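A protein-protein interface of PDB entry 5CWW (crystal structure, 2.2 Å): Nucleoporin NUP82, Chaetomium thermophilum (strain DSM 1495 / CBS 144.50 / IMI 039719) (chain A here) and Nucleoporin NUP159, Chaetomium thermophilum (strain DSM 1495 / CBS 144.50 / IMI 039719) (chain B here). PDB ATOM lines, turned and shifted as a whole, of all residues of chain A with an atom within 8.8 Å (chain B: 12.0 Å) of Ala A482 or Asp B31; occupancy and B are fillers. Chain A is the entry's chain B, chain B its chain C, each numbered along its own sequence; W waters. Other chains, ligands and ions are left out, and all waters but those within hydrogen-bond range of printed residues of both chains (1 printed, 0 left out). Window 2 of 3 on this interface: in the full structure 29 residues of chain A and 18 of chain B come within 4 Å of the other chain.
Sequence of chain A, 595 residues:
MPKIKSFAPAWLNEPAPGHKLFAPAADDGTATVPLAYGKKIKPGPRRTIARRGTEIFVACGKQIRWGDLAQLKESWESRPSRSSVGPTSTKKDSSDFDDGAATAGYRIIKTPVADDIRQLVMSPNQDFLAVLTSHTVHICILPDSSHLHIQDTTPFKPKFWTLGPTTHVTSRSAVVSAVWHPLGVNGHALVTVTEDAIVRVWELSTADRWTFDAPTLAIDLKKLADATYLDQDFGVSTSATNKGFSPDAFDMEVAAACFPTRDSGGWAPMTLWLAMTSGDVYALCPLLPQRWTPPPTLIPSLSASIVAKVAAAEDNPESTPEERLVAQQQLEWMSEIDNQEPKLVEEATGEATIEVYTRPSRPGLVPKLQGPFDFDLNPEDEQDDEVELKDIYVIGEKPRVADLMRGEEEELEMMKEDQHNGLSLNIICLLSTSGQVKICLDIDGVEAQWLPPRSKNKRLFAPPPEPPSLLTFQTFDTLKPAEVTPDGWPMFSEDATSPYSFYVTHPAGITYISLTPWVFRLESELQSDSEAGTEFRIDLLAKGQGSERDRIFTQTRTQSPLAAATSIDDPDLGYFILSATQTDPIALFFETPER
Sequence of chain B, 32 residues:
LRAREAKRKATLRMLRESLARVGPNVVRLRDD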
ATOM      1  N   SER A 434      17.081  13.538  21.120  1.00  0.00           N
ATOM      2  CA  SER A 434      15.787  14.138  21.421  1.00  0.00           C
ATOM      3  C   SER A 434      14.974  14.402  20.160  1.00  0.00           C
ATOM      4  O   SER A 434      13.788  14.717  20.238  1.00  0.00           O
ATOM      5  CB  SER A 434      15.973  15.447  22.186  1.00  0.00           C
ATOM      6  OG  SER A 434      16.555  16.435  21.354  1.00  0.00           O
ATOM      7  N   ASP A 477      13.217  21.575  17.401  1.00  0.00           N
ATOM      8  CA  ASP A 477      12.711  20.253  17.747  1.00  0.00           C
ATOM      9  C   ASP A 477      11.919  19.658  16.591  1.00  0.00           C
ATOM     10  O   ASP A 477      11.364  20.387  15.766  1.00  0.00           O
ATOM     11  CB  ASP A 477      11.821  20.314  18.994  1.00  0.00           C
ATOM     12  CG  ASP A 477      12.609  20.517  20.277  1.00  0.00           C
ATOM     13  OD1 ASP A 477      13.767  20.055  20.355  1.00  0.00           O
ATOM     14  OD2 ASP A 477      12.056  21.121  21.218  1.00  0.00           O
ATOM     15  N   LEU A 479      10.302  16.585  17.723  1.00  0.00           N
ATOM     16  CA  LEU A 479       9.469  15.781  18.617  1.00  0.00           C
ATOM     17  C   LEU A 479       8.961  16.608  19.792  1.00  0.00           C
ATOM     18  O   LEU A 479       9.624  17.544  20.237  1.00  0.00           O
ATOM     19  CB  LEU A 479      10.251  14.578  19.149  1.00  0.00           C
ATOM     20  CG  LEU A 479      10.754  13.553  18.131  1.00  0.00           C
ATOM     21  CD1 LEU A 479      11.607  12.501  18.828  1.00  0.00           C
ATOM     22  CD2 LEU A 479       9.594  12.902  17.401  1.00  0.00           C
ATOM     23  N   LYS A 480       7.782  16.254  20.293  1.00  0.00           N
ATOM     24  CA  LYS A 480       7.293  16.826  21.539  1.00  0.00           C
ATOM     25  C   LYS A 480       8.000  16.112  22.687  1.00  0.00           C
ATOM     26  O   LYS A 480       8.459  14.985  22.514  1.00  0.00           O
ATOM     27  CB  LYS A 480       5.776  16.676  21.670  1.00  0.00           C
ATOM     28  CG  LYS A 480       4.983  17.155  20.468  1.00  0.00           C
ATOM     29  CD  LYS A 480       3.508  17.308  20.815  1.00  0.00           C
ATOM     30  CE  LYS A 480       2.657  17.543  19.579  1.00  0.00           C
ATOM     31  NZ  LYS A 480       2.605  16.339  18.702  1.00  0.00           N
ATOM     32  N   PRO A 481       8.097  16.764  23.857  1.00  0.00           N
ATOM     33  CA  PRO A 481       8.767  16.160  25.016  1.00  0.00           C
ATOM     34  C   PRO A 481       8.250  14.761  25.350  1.00  0.00           C
ATOM     35  O   PRO A 481       9.029  13.891  25.737  1.00  0.00           O
ATOM     36  CB  PRO A 481       8.450  17.139  26.147  1.00  0.00           C
ATOM     37  CG  PRO A 481       8.270  18.448  25.468  1.00  0.00           C
ATOM     38  CD  PRO A 481       7.639  18.136  24.141  1.00  0.00           C
ATOM     39  N   ALA A 482       6.947  14.554  25.186  1.00  0.00           N
ATOM     40  CA  ALA A 482       6.321  13.273  25.499  1.00  0.00           C
ATOM     41  C   ALA A 482       6.700  12.191  24.490  1.00  0.00           C
ATOM     42  O   ALA A 482       6.537  11.001  24.758  1.00  0.00           O
ATOM     43  CB  ALA A 482       4.811  13.431  25.556  1.00  0.00           C
ATOM     44  N   GLU A 483       7.204  12.610  23.332  1.00  0.00           N
ATOM     45  CA  GLU A 483       7.549  11.680  22.260  1.00  0.00           C
ATOM     46  C   GLU A 483       9.002  11.222  22.339  1.00  0.00           C
ATOM     47  O   GLU A 483       9.388  10.243  21.699  1.00  0.00           O
ATOM     48  CB  GLU A 483       7.284  12.323  20.899  1.00  0.00           C
ATOM     49  CG  GLU A 483       5.821  12.634  20.643  1.00  0.00           C
ATOM     50  CD  GLU A 483       5.593  13.285  19.297  1.00  0.00           C
ATOM     51  OE1 GLU A 483       6.228  14.323  19.018  1.00  0.00           O
ATOM     52  OE2 GLU A 483       4.783  12.752  18.508  1.00  0.00           O
ATOM     53  N   VAL A 484       9.804  11.933  23.124  1.00  0.00           N
ATOM     54  CA  VAL A 484      11.225  11.631  23.243  1.00  0.00           C
ATOM     55  C   VAL A 484      11.459  10.354  24.041  1.00  0.00           C
ATOM     56  O   VAL A 484      11.044  10.250  25.195  1.00  0.00           O
ATOM     57  CB  VAL A 484      11.993  12.788  23.918  1.00  0.00           C
ATOM     58  CG1 VAL A 484      13.482  12.471  24.008  1.00  0.00           C
ATOM     59  CG2 VAL A 484      11.772  14.087  23.161  1.00  0.00           C
ATOM     60  N   THR A 485      12.125   9.387  23.416  1.00  0.00           N
ATOM     61  CA  THR A 485      12.548   8.169  24.099  1.00  0.00           C
ATOM     62  C   THR A 485      14.022   8.313  24.479  1.00  0.00           C
ATOM     63  O   THR A 485      14.805   8.871  23.711  1.00  0.00           O
ATOM     64  CB  THR A 485      12.350   6.915  23.225  1.00  0.00           C
ATOM     65  OG1 THR A 485      13.141   7.022  22.036  1.00  0.00           O
ATOM     66  CG2 THR A 485      10.886   6.753  22.843  1.00  0.00           C
ATOM     67  N   PRO A 486      14.406   7.809  25.664  1.00  0.00           N
ATOM     68  CA  PRO A 486      15.757   8.057  26.187  1.00  0.00           C
ATOM     69  C   PRO A 486      16.865   7.447  25.330  1.00  0.00           C
ATOM     70  O   PRO A 486      17.979   7.974  25.307  1.00  0.00           O
ATOM     71  CB  PRO A 486      15.721   7.400  27.572  1.00  0.00           C
ATOM     72  CG  PRO A 486      14.680   6.343  27.462  1.00  0.00           C
ATOM     73  CD  PRO A 486      13.643   6.885  26.522  1.00  0.00           C
ATOM     74  N   HIS A 506      11.574   8.569  13.136  1.00  0.00           N
ATOM     75  CA  HIS A 506      11.669   8.251  14.555  1.00  0.00           C
ATOM     76  C   HIS A 506      10.446   7.404  14.894  1.00  0.00           C
ATOM     77  O   HIS A 506       9.421   7.522  14.221  1.00  0.00           O
ATOM     78  CB  HIS A 506      11.721   9.538  15.388  1.00  0.00           C
ATOM     79  CG  HIS A 506      11.972   9.318  16.847  1.00  0.00           C
ATOM     80  ND1 HIS A 506      10.955   9.139  17.759  1.00  0.00           N
ATOM     81  CD2 HIS A 506      13.125   9.264  17.555  1.00  0.00           C
ATOM     82  CE1 HIS A 506      11.469   8.974  18.964  1.00  0.00           C
ATOM     83  NE2 HIS A 506      12.785   9.047  18.868  1.00  0.00           N
ATOM     84  N   ALA A 508       8.282   7.834  16.887  1.00  0.00           N
ATOM     85  CA  ALA A 508       7.158   8.719  17.165  1.00  0.00           C
ATOM     86  C   ALA A 508       6.487   9.183  15.875  1.00  0.00           C
ATOM     87  O   ALA A 508       5.281   9.424  15.849  1.00  0.00           O
ATOM     88  CB  ALA A 508       7.618   9.917  17.980  1.00  0.00           C
ATOM     89  N   ARG A 551       5.177  17.725   9.934  1.00  0.00           N
ATOM     90  CA  ARG A 551       5.011  16.314  10.234  1.00  0.00           C
ATOM     91  C   ARG A 551       4.023  15.679   9.270  1.00  0.00           C
ATOM     92  O   ARG A 551       2.917  16.182   9.074  1.00  0.00           O
ATOM     93  CB  ARG A 551       4.539  16.109  11.669  1.00  0.00           C
ATOM     94  CG  ARG A 551       4.346  14.646  12.005  1.00  0.00           C
ATOM     95  CD  ARG A 551       4.357  14.393  13.495  1.00  0.00           C
ATOM     96  NE  ARG A 551       5.600  14.812  14.131  1.00  0.00           N
ATOM     97  CZ  ARG A 551       5.942  14.479  15.370  1.00  0.00           C
ATOM     98  NH1 ARG A 551       7.085  14.904  15.880  1.00  0.00           N
ATOM     99  NH2 ARG A 551       5.140  13.715  16.100  1.00  0.00           N
ATOM    100  N   VAL B  27      13.815  26.937  18.173  1.00  0.00           N
ATOM    101  CA  VAL B  27      12.376  26.696  18.132  1.00  0.00           C
ATOM    102  C   VAL B  27      12.051  25.335  18.731  1.00  0.00           C
ATOM    103  O   VAL B  27      12.207  24.307  18.069  1.00  0.00           O
ATOM    104  CB  VAL B  27      11.834  26.755  16.688  1.00  0.00           C
ATOM    105  CG1 VAL B  27      10.325  26.534  16.667  1.00  0.00           C
ATOM    106  CG2 VAL B  27      12.186  28.088  16.041  1.00  0.00           C
ATOM    107  N   ARG B  28      11.592  25.327  19.979  1.00  0.00           N
ATOM    108  CA  ARG B  28      11.278  24.079  20.665  1.00  0.00           C
ATOM    109  C   ARG B  28       9.777  23.799  20.661  1.00  0.00           C
ATOM    110  O   ARG B  28       8.967  24.717  20.536  1.00  0.00           O
ATOM    111  CB  ARG B  28      11.804  24.120  22.103  1.00  0.00           C
ATOM    112  CG  ARG B  28      13.325  24.086  22.201  1.00  0.00           C
ATOM    113  CD  ARG B  28      13.794  23.630  23.572  1.00  0.00           C
ATOM    114  NE  ARG B  28      15.234  23.385  23.606  1.00  0.00           N
ATOM    115  CZ  ARG B  28      16.154  24.306  23.883  1.00  0.00           C
ATOM    116  NH1 ARG B  28      15.800  25.555  24.152  1.00  0.00           N
ATOM    117  NH2 ARG B  28      17.439  23.975  23.887  1.00  0.00           N
ATOM    118  N   LEU B  29       9.421  22.525  20.791  1.00  0.00           N
ATOM    119  CA  LEU B  29       8.024  22.098  20.753  1.00  0.00           C
ATOM    120  C   LEU B  29       7.481  21.800  22.146  1.00  0.00           C
ATOM    121  O   LEU B  29       8.154  21.167  22.960  1.00  0.00           O
ATOM    122  CB  LEU B  29       7.870  20.860  19.866  1.00  0.00           C
ATOM    123  CG  LEU B  29       8.166  21.055  18.378  1.00  0.00           C
ATOM    124  CD1 LEU B  29       8.149  19.718  17.657  1.00  0.00           C
ATOM    125  CD2 LEU B  29       7.162  22.013  17.752  1.00  0.00           C
ATOM    126  N   ARG B  30       6.265  22.267  22.411  1.00  0.00           N
ATOM    127  CA  ARG B  30       5.559  21.935  23.643  1.00  0.00           C
ATOM    128  C   ARG B  30       4.643  20.733  23.428  1.00  0.00           C
ATOM    129  O   ARG B  30       4.374  20.341  22.291  1.00  0.00           O
ATOM    130  CB  ARG B  30       4.741  23.131  24.135  1.00  0.00           C
ATOM    131  CG  ARG B  30       5.573  24.321  24.587  1.00  0.00           C
ATOM    132  CD  ARG B  30       5.873  25.278  23.441  1.00  0.00           C
ATOM    133  NE  ARG B  30       6.309  26.585  23.926  1.00  0.00           N
ATOM    134  CZ  ARG B  30       6.539  27.638  23.146  1.00  0.00           C
ATOM    135  NH1 ARG B  30       6.377  27.548  21.833  1.00  0.00           N
ATOM    136  NH2 ARG B  30       6.930  28.787  23.682  1.00  0.00           N
ATOM    137  N   ASP B  31       4.169  20.152  24.525  1.00  0.00           N
ATOM    138  CA  ASP B  31       3.239  19.030  24.460  1.00  0.00           C
ATOM    139  C   ASP B  31       1.906  19.464  23.855  1.00  0.00           C
ATOM    140  O   ASP B  31       1.369  18.804  22.966  1.00  0.00           O
ATOM    141  CB  ASP B  31       3.024  18.434  25.851  1.00  0.00           C
ATOM    142  CG  ASP B  31       4.267  17.753  26.392  1.00  0.00           C
ATOM    143  OD1 ASP B  31       4.878  16.953  25.654  1.00  0.00           O
ATOM    144  OD2 ASP B  31       4.635  18.023  27.554  1.00  0.00           O
ATOM    145  N   ASP B  32       1.377  20.582  24.348  1.00  0.00           N
ATOM    146  CA  ASP B  32       0.122  21.132  23.848  1.00  0.00           C
ATOM    147  C   ASP B  32       0.117  22.653  23.961  1.00  0.00           C
ATOM    148  O   ASP B  32       0.182  23.360  22.957  1.00  0.00           O
ATOM    149  CB  ASP B  32      -1.069  20.551  24.615  1.00  0.00           C
ATOM    150  CG  ASP B  32      -1.222  19.056  24.412  1.00  0.00           C
ATOM    151  OD1 ASP B  32      -1.905  18.651  23.449  1.00  0.00           O
ATOM    152  OD2 ASP B  32      -0.658  18.285  25.218  1.00  0.00           O
HETATM  153  O   HOH W   1      16.114  21.694  21.078  1.00  0.00           O
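Asp A477 touches Arg B28.
Leu A479 touches Leu B29 (O to CD1, 3.7 Å).
Arg B30 touches Lys A480 (O to CD, 3.5 Å).
Lys A480 touches Asp B31 (CD to O, 3.4 Å).
Pro A481 touches Leu B29.
Pro A481 touches Asp B31.
Water W1 lies within hydrogen-bond range of OD1 of Asp A477 (3.0 Å) and NE of Arg B28 (3.2 Å).
The backbone carbonyl oxygen (O) of Val B27 is in hydrogen-bond range of the backbone NH (N) of Asp A477.
OD2 of Asp A477 sits at hydrogen-bond distance from N of Leu B29 (3.0 Å).
N of Ala A482 sits at hydrogen-bond distance from OD1 of Asp B31, at 3.2 Å.
Hydrophobic or aromatic side chains of chain A within 4 Å of the printed part of chain B: Pro A481 and Ala A482.
Printed residues of chain B that touch a printed residue of chain A: Val B27, Arg B28, Leu B29, Arg B30 and Asp B31.
Among the printed residues, 9 pairs touch across the chains.
Among the printed residues, no Asp or Glu carboxylate lies within 4 Å of a Lys or Arg side-chain nitrogen of the other chain.
N of Lys A480 lies within hydrogen-bond range of OE1 of Glu A483 (2.8 Å).
Of chain B, only Asp B31 comes within 4 Å of Ala A482.
Of chain A, only Lys A480, Pro A481 and Ala A482 come within 4 Å of Asp B31.
Pro A481 touches just these residues of chain B: Leu B29 (3.3 Å) and Asp B31 (3.4 Å).
No residue of chain B comes within 4 Å of Glu A483.
No residue of chain A comes within 4 Å of Asp B32.
Of the printed residues of chain A, Arg B30 touches Lys A480 (3.5 Å).
Of the printed residues of chain B, Leu A479 touches Leu B29.
Printed residues of chain A within 4 Å of Val B27: Asp A477.
The nearest printed residue of chain A that does not touch Val B27 is Leu A479 (7.6 Å).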
